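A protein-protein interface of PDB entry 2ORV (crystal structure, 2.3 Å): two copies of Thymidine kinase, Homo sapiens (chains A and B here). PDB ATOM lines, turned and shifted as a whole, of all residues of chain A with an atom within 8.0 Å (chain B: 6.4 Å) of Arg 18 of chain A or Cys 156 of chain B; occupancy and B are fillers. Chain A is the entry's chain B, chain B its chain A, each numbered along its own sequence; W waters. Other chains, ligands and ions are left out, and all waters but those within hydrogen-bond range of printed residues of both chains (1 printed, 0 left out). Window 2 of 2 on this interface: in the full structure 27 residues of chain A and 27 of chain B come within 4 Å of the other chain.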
ATOM      1  N   ARG A  18      -3.502  -6.486 -11.062  1.00  0.00           N
ATOM      2  CA  ARG A  18      -4.098  -5.817  -9.850  1.00  0.00           C
ATOM      3  C   ARG A  18      -3.030  -5.287  -8.830  1.00  0.00           C
ATOM      4  O   ARG A  18      -2.239  -6.061  -8.250  1.00  0.00           O
ATOM      5  CB  ARG A  18      -5.222  -6.677  -9.198  1.00  0.00           C
ATOM      6  CG  ARG A  18      -5.199  -8.213  -9.485  1.00  0.00           C
ATOM      7  CD  ARG A  18      -6.127  -9.046  -8.500  1.00  0.00           C
ATOM      8  NE  ARG A  18      -7.452  -9.438  -9.048  1.00  0.00           N
ATOM      9  CZ  ARG A  18      -8.657  -9.147  -8.510  1.00  0.00           C
ATOM     10  NH1 ARG A  18      -8.761  -8.446  -7.373  1.00  0.00           N
ATOM     11  NH2 ARG A  18      -9.780  -9.564  -9.117  1.00  0.00           N
ATOM     12  N   GLY A  19      -3.003  -3.952  -8.674  1.00  0.00           N
ATOM     13  CA  GLY A  19      -2.072  -3.271  -7.782  1.00  0.00           C
ATOM     14  C   GLY A  19      -2.689  -3.002  -6.417  1.00  0.00           C
ATOM     15  O   GLY A  19      -3.913  -3.150  -6.238  1.00  0.00           O
ATOM     16  N   GLN A  20      -1.852  -2.582  -5.460  1.00  0.00           N
ATOM     17  CA  GLN A  20      -2.295  -2.357  -4.090  1.00  0.00           C
ATOM     18  C   GLN A  20      -1.382  -1.397  -3.321  1.00  0.00           C
ATOM     19  O   GLN A  20      -0.326  -1.011  -3.822  1.00  0.00           O
ATOM     20  CB  GLN A  20      -2.345  -3.686  -3.351  1.00  0.00           C
ATOM     21  CG  GLN A  20      -0.990  -4.212  -3.078  1.00  0.00           C
ATOM     22  CD  GLN A  20      -1.036  -5.605  -2.556  1.00  0.00           C
ATOM     23  OE1 GLN A  20      -1.251  -6.547  -3.319  1.00  0.00           O
ATOM     24  NE2 GLN A  20      -0.825  -5.763  -1.256  1.00  0.00           N
ATOM     25  N   ILE A  21      -1.809  -1.017  -2.113  1.00  0.00           N
ATOM     26  CA  ILE A  21      -1.031  -0.189  -1.196  1.00  0.00           C
ATOM     27  C   ILE A  21      -1.036  -0.805   0.209  1.00  0.00           C
ATOM     28  O   ILE A  21      -2.088  -0.974   0.780  1.00  0.00           O
ATOM     29  CB  ILE A  21      -1.588   1.248  -1.117  1.00  0.00           C
ATOM     30  CG1 ILE A  21      -1.656   1.890  -2.497  1.00  0.00           C
ATOM     31  CG2 ILE A  21      -0.733   2.122  -0.191  1.00  0.00           C
ATOM     32  CD1 ILE A  21      -2.271   3.267  -2.494  1.00  0.00           C
ATOM     33  N   ALA A  92       7.741  -3.490 -10.823  1.00  0.00           N
ATOM     34  CA  ALA A  92       6.550  -4.170 -10.298  1.00  0.00           C
ATOM     35  C   ALA A  92       6.236  -3.807  -8.825  1.00  0.00           C
ATOM     36  O   ALA A  92       5.075  -3.596  -8.471  1.00  0.00           O
ATOM     37  CB  ALA A  92       6.698  -5.660 -10.469  1.00  0.00           C
ATOM     38  N   MET A 112       0.515   4.917  -8.731  1.00  0.00           N
ATOM     39  CA  MET A 112       1.241   3.660  -8.871  1.00  0.00           C
ATOM     40  C   MET A 112       0.338   2.426  -8.744  1.00  0.00           C
ATOM     41  O   MET A 112       0.415   1.529  -9.585  1.00  0.00           O
ATOM     42  CB  MET A 112       2.438   3.575  -7.931  1.00  0.00           C
ATOM     43  CG  MET A 112       3.597   4.480  -8.329  1.00  0.00           C
ATOM     44  SD  MET A 112       4.031   4.508 -10.101  1.00  0.00           S
ATOM     45  CE  MET A 112       4.549   6.231 -10.197  1.00  0.00           C
ATOM     46  N   ALA A 113      -0.526   2.382  -7.717  1.00  0.00           N
ATOM     47  CA  ALA A 113      -1.307   1.166  -7.438  1.00  0.00           C
ATOM     48  C   ALA A 113      -2.330   0.956  -8.532  1.00  0.00           C
ATOM     49  O   ALA A 113      -2.561  -0.170  -9.002  1.00  0.00           O
ATOM     50  CB  ALA A 113      -1.970   1.258  -6.095  1.00  0.00           C
ATOM     51  N   ASN A 114      -2.944   2.063  -8.930  1.00  0.00           N
ATOM     52  CA  ASN A 114      -3.795   2.072 -10.105  1.00  0.00           C
ATOM     53  C   ASN A 114      -3.055   1.757 -11.446  1.00  0.00           C
ATOM     54  O   ASN A 114      -3.658   1.178 -12.359  1.00  0.00           O
ATOM     55  CB  ASN A 114      -4.610   3.358 -10.143  1.00  0.00           C
ATOM     56  CG  ASN A 114      -5.717   3.358  -9.097  1.00  0.00           C
ATOM     57  OD1 ASN A 114      -5.970   4.376  -8.455  1.00  0.00           O
ATOM     58  ND2 ASN A 114      -6.375   2.196  -8.902  1.00  0.00           N
ATOM     59  N   ALA A 115      -1.762   2.088 -11.545  1.00  0.00           N
ATOM     60  CA  ALA A 115      -0.908   1.542 -12.603  1.00  0.00           C
ATOM     61  C   ALA A 115      -0.692   0.004 -12.526  1.00  0.00           C
ATOM     62  O   ALA A 115      -0.068  -0.582 -13.405  1.00  0.00           O
ATOM     63  CB  ALA A 115       0.431   2.255 -12.598  1.00  0.00           C
ATOM     64  N   GLY A 116      -1.164  -0.658 -11.472  1.00  0.00           N
ATOM     65  CA  GLY A 116      -0.918  -2.109 -11.332  1.00  0.00           C
ATOM     66  C   GLY A 116       0.278  -2.545 -10.504  1.00  0.00           C
ATOM     67  O   GLY A 116       0.635  -3.715 -10.502  1.00  0.00           O
ATOM     68  N   LYS A 117       0.890  -1.611  -9.781  1.00  0.00           N
ATOM     69  CA  LYS A 117       2.050  -1.898  -8.924  1.00  0.00           C
ATOM     70  C   LYS A 117       1.713  -2.212  -7.435  1.00  0.00           C
ATOM     71  O   LYS A 117       0.774  -1.642  -6.865  1.00  0.00           O
ATOM     72  CB  LYS A 117       2.981  -0.687  -8.933  1.00  0.00           C
ATOM     73  CG  LYS A 117       3.910  -0.592 -10.118  1.00  0.00           C
ATOM     74  CD  LYS A 117       3.424   0.456 -11.111  1.00  0.00           C
ATOM     75  CE  LYS A 117       4.526   0.759 -12.135  1.00  0.00           C
ATOM     76  NZ  LYS A 117       4.776  -0.401 -13.074  1.00  0.00           N
ATOM     77  N   THR A 118       2.510  -3.078  -6.802  1.00  0.00           N
ATOM     78  CA  THR A 118       2.502  -3.242  -5.357  1.00  0.00           C
ATOM     79  C   THR A 118       3.361  -2.168  -4.688  1.00  0.00           C
ATOM     80  O   THR A 118       4.582  -2.127  -4.862  1.00  0.00           O
ATOM     81  CB  THR A 118       2.987  -4.636  -4.974  1.00  0.00           C
ATOM     82  OG1 THR A 118       2.113  -5.589  -5.568  1.00  0.00           O
ATOM     83  CG2 THR A 118       2.966  -4.848  -3.468  1.00  0.00           C
ATOM     84  N   GLU A 144      -4.915  -1.254   1.015  1.00  0.00           N
ATOM     85  CA  GLU A 144      -5.459  -2.584   1.169  1.00  0.00           C
ATOM     86  C   GLU A 144      -5.069  -3.162   2.508  1.00  0.00           C
ATOM     87  O   GLU A 144      -5.794  -3.992   3.072  1.00  0.00           O
ATOM     88  CB  GLU A 144      -4.967  -3.490   0.063  1.00  0.00           C
ATOM     89  CG  GLU A 144      -5.853  -3.452  -1.197  1.00  0.00           C
ATOM     90  CD  GLU A 144      -5.519  -2.347  -2.215  1.00  0.00           C
ATOM     91  OE1 GLU A 144      -4.920  -1.277  -1.870  1.00  0.00           O
ATOM     92  OE2 GLU A 144      -5.934  -2.537  -3.382  1.00  0.00           O
ATOM     93  N   CYS B 153     -14.948  -9.237  -1.660  1.00  0.00           N
ATOM     94  CA  CYS B 153     -15.560  -8.439  -2.705  1.00  0.00           C
ATOM     95  C   CYS B 153     -16.888  -9.050  -3.128  1.00  0.00           C
ATOM     96  O   CYS B 153     -16.967 -10.233  -3.428  1.00  0.00           O
ATOM     97  CB  CYS B 153     -14.639  -8.262  -3.911  1.00  0.00           C
ATOM     98  SG  CYS B 153     -15.345  -7.077  -5.080  1.00  0.00           S
ATOM     99  N   MET B 154     -17.926  -8.226  -3.124  1.00  0.00           N
ATOM    100  CA  MET B 154     -19.261  -8.678  -3.484  1.00  0.00           C
ATOM    101  C   MET B 154     -19.431  -8.760  -5.017  1.00  0.00           C
ATOM    102  O   MET B 154     -20.450  -9.209  -5.486  1.00  0.00           O
ATOM    103  CB  MET B 154     -20.323  -7.766  -2.846  1.00  0.00           C
ATOM    104  CG  MET B 154     -20.641  -8.111  -1.397  1.00  0.00           C
ATOM    105  SD  MET B 154     -21.606  -6.841  -0.520  1.00  0.00           S
ATOM    106  CE  MET B 154     -21.716  -7.626   1.086  1.00  0.00           C
ATOM    107  N   GLU B 155     -18.426  -8.351  -5.794  1.00  0.00           N
ATOM    108  CA  GLU B 155     -18.552  -8.357  -7.245  1.00  0.00           C
ATOM    109  C   GLU B 155     -17.582  -9.275  -7.981  1.00  0.00           C
ATOM    110  O   GLU B 155     -17.914  -9.773  -9.051  1.00  0.00           O
ATOM    111  CB  GLU B 155     -18.498  -6.936  -7.803  1.00  0.00           C
ATOM    112  CG  GLU B 155     -19.780  -6.179  -7.603  1.00  0.00           C
ATOM    113  CD  GLU B 155     -19.602  -4.662  -7.575  1.00  0.00           C
ATOM    114  OE1 GLU B 155     -18.823  -4.112  -8.396  1.00  0.00           O
ATOM    115  OE2 GLU B 155     -20.280  -4.000  -6.741  1.00  0.00           O
ATOM    116  N   CYS B 156     -16.394  -9.520  -7.435  1.00  0.00           N
ATOM    117  CA  CYS B 156     -15.443 -10.456  -8.079  1.00  0.00           C
ATOM    118  C   CYS B 156     -14.983 -11.568  -7.135  1.00  0.00           C
ATOM    119  O   CYS B 156     -14.386 -12.565  -7.568  1.00  0.00           O
ATOM    120  CB  CYS B 156     -14.223  -9.703  -8.612  1.00  0.00           C
ATOM    121  SG  CYS B 156     -13.128  -9.067  -7.306  1.00  0.00           S
ATOM    122  N   PHE B 157     -15.241 -11.385  -5.841  1.00  0.00           N
ATOM    123  CA  PHE B 157     -14.866 -12.369  -4.810  1.00  0.00           C
ATOM    124  C   PHE B 157     -13.349 -12.462  -4.459  1.00  0.00           C
ATOM    125  O   PHE B 157     -12.874 -13.495  -3.986  1.00  0.00           O
ATOM    126  CB  PHE B 157     -15.464 -13.760  -5.135  1.00  0.00           C
ATOM    127  CG  PHE B 157     -16.849 -13.702  -5.768  1.00  0.00           C
ATOM    128  CD1 PHE B 157     -17.052 -14.158  -7.084  1.00  0.00           C
ATOM    129  CD2 PHE B 157     -17.934 -13.165  -5.061  1.00  0.00           C
ATOM    130  CE1 PHE B 157     -18.305 -14.081  -7.683  1.00  0.00           C
ATOM    131  CE2 PHE B 157     -19.189 -13.077  -5.645  1.00  0.00           C
ATOM    132  CZ  PHE B 157     -19.377 -13.538  -6.967  1.00  0.00           C
ATOM    133  N   ARG B 158     -12.600 -11.380  -4.673  1.00  0.00           N
ATOM    134  CA  ARG B 158     -11.266 -11.257  -4.076  1.00  0.00           C
ATOM    135  C   ARG B 158     -11.451 -10.661  -2.673  1.00  0.00           C
ATOM    136  O   ARG B 158     -12.578 -10.540  -2.205  1.00  0.00           O
ATOM    137  CB  ARG B 158     -10.364 -10.387  -4.950  1.00  0.00           C
ATOM    138  CG  ARG B 158     -10.241 -10.876  -6.392  1.00  0.00           C
ATOM    139  CD  ARG B 158      -9.646 -12.299  -6.499  1.00  0.00           C
ATOM    140  NE  ARG B 158      -9.707 -12.859  -7.858  1.00  0.00           N
ATOM    141  CZ  ARG B 158     -10.510 -13.855  -8.242  1.00  0.00           C
ATOM    142  NH1 ARG B 158     -11.360 -14.426  -7.375  1.00  0.00           N
ATOM    143  NH2 ARG B 158     -10.472 -14.275  -9.504  1.00  0.00           N
ATOM    144  N   GLU B 159     -10.374 -10.311  -1.986  1.00  0.00           N
ATOM    145  CA  GLU B 159     -10.527  -9.618  -0.716  1.00  0.00           C
ATOM    146  C   GLU B 159     -10.979  -8.173  -1.005  1.00  0.00           C
ATOM    147  O   GLU B 159     -10.602  -7.592  -2.037  1.00  0.00           O
ATOM    148  CB  GLU B 159      -9.222  -9.657   0.083  1.00  0.00           C
ATOM    149  CG  GLU B 159      -8.924 -11.046   0.664  1.00  0.00           C
ATOM    150  CD  GLU B 159      -7.780 -11.051   1.712  1.00  0.00           C
ATOM    151  OE1 GLU B 159      -6.744 -10.355   1.487  1.00  0.00           O
ATOM    152  OE2 GLU B 159      -7.934 -11.764   2.757  1.00  0.00           O
ATOM    153  N   CYS B 185     -13.092  -4.656  -3.695  1.00  0.00           N
ATOM    154  CA  CYS B 185     -11.673  -4.448  -4.020  1.00  0.00           C
ATOM    155  C   CYS B 185     -11.441  -3.201  -4.901  1.00  0.00           C
ATOM    156  O   CYS B 185     -12.386  -2.607  -5.396  1.00  0.00           O
ATOM    157  CB  CYS B 185     -11.098  -5.659  -4.730  1.00  0.00           C
ATOM    158  SG  CYS B 185     -11.667  -5.758  -6.465  1.00  0.00           S
ATOM    159  N   ARG B 186     -10.170  -2.835  -5.077  1.00  0.00           N
ATOM    160  CA  ARG B 186      -9.713  -1.714  -5.917  1.00  0.00           C
ATOM    161  C   ARG B 186     -10.265  -1.807  -7.339  1.00  0.00           C
ATOM    162  O   ARG B 186     -10.799  -0.847  -7.878  1.00  0.00           O
ATOM    163  CB  ARG B 186      -8.175  -1.716  -5.962  1.00  0.00           C
ATOM    164  CG  ARG B 186      -7.537  -0.596  -6.803  1.00  0.00           C
ATOM    165  CD  ARG B 186      -6.008  -0.532  -6.667  1.00  0.00           C
ATOM    166  NE  ARG B 186      -5.542  -0.210  -5.315  1.00  0.00           N
ATOM    167  CZ  ARG B 186      -5.397   1.020  -4.810  1.00  0.00           C
ATOM    168  NH1 ARG B 186      -5.690   2.122  -5.520  1.00  0.00           N
ATOM    169  NH2 ARG B 186      -4.937   1.152  -3.574  1.00  0.00           N
ATOM    170  N   LEU B 187     -10.114  -2.979  -7.946  1.00  0.00           N
ATOM    171  CA  LEU B 187     -10.628  -3.210  -9.289  1.00  0.00           C
ATOM    172  C   LEU B 187     -12.119  -2.926  -9.420  1.00  0.00           C
ATOM    173  O   LEU B 187     -12.518  -2.091 -10.234  1.00  0.00           O
ATOM    174  CB  LEU B 187     -10.305  -4.616  -9.759  1.00  0.00           C
ATOM    175  CG  LEU B 187      -9.293  -4.610 -10.890  1.00  0.00           C
ATOM    176  CD1 LEU B 187      -8.250  -5.712 -10.678  1.00  0.00           C
ATOM    177  CD2 LEU B 187     -10.050  -4.771 -12.239  1.00  0.00           C
ATOM    178  N   CYS B 188     -12.937  -3.589  -8.599  1.00  0.00           N
ATOM    179  CA  CYS B 188     -14.389  -3.418  -8.685  1.00  0.00           C
ATOM    180  C   CYS B 188     -14.819  -2.034  -8.272  1.00  0.00           C
ATOM    181  O   CYS B 188     -15.737  -1.495  -8.849  1.00  0.00           O
ATOM    182  CB  CYS B 188     -15.126  -4.474  -7.878  1.00  0.00           C
ATOM    183  SG  CYS B 188     -14.875  -6.128  -8.513  1.00  0.00           S
HETATM  184  O   HOH W   1      -7.677  -4.390  -3.947  1.00  0.00           O
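The guanidinium group (NE) of Arg 186 of chain B sits close to the backbone carbonyl oxygen (O) of Gly 19 of chain A (3.5 Å).
The side-chain amide nitrogen of Asn 114 of chain A lies close to the guanidinium group of Arg 186 of chain B, 3.5 Å away.
NH2 of Arg 186 of chain B lies within salt-bridge range of OE1 of Glu 144 of chain A (3.0 Å).
The backbone NH (N) of Cys 153 of chain B sits at hydrogen-bond distance from the backbone carbonyl oxygen (O) of Arg 158 of chain B, 2.8 Å away.
The side-chain sulfur (SG) of Cys 156 of chain B lies close to the backbone NH (N) of Arg 158 of chain B.
SG of Cys 185 of chain B lies close to N of Leu 187 of chain B.
The backbone carbonyl oxygen of Ile 21 of chain A sits at hydrogen-bond distance from the backbone NH of Glu 144 of chain A (2.9 Å).
Cys 156 of chain B touches Arg 18 of chain A (SG to NH2, 3.8 Å).
Arg 158 of chain B touches Arg 18 of chain A.
CB of Arg 18 of chain A touches CD1 of Leu 187 of chain B, at 3.5 Å.
CG1 of Ile 21 of chain A touches NH2 of Arg 186 of chain B, at 3.5 Å.
Ala 113 of chain A touches Arg 186 of chain B (CB to CZ, 3.7 Å).
Of the printed residues of chain B, Arg 18 of chain A touches Cys 156, Arg 158 and Leu 187.
Printed residues of chain B within 4 Å of Ile 21 of chain A: Arg 186.
Met 112 of chain A touches none of the printed residues of chain B.
Printed residues of chain B within 4 Å of Ala 113 of chain A: Arg 186.
Lys 117 of chain A touches none of the printed residues of chain B.
Cys 156 of chain B touches one residue of chain A.
Printed residues of chain A within 4 Å of Arg 158 of chain B: Arg 18 (3.0 Å).
Printed residues of chain A within 4 Å of Arg 186 of chain B: Gly 19 (3.4 Å), Ile 21 (3.5 Å), Ala 113 (3.7 Å), Asn 114 (3.5 Å) and Glu 144 (3.0 Å).
The nearest printed residue of chain A that does not touch Cys 156 of chain B is Glu 144 of chain A (10.5 Å).
Of the 13 printed residues of chain A, 6 touch a printed residue of chain B.
Hydrophobic or aromatic side chains of chain A that line the printed part of chain B: Ile 21 and Ala 113.
Of the 11 printed residues of chain B, 4 touch a printed residue of chain A.
Among the printed residues, 8 pairs touch across the chains.
No position is printed for both chains.
Of the 8 pairs that touch across the chains among the printed residues, none has its exchanged pair printed and touching as well.
Water W1 bridges the side-chain carboxylate (OE2) of Glu 144 of chain A and the backbone NH (N) of Arg 186 of chain B.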
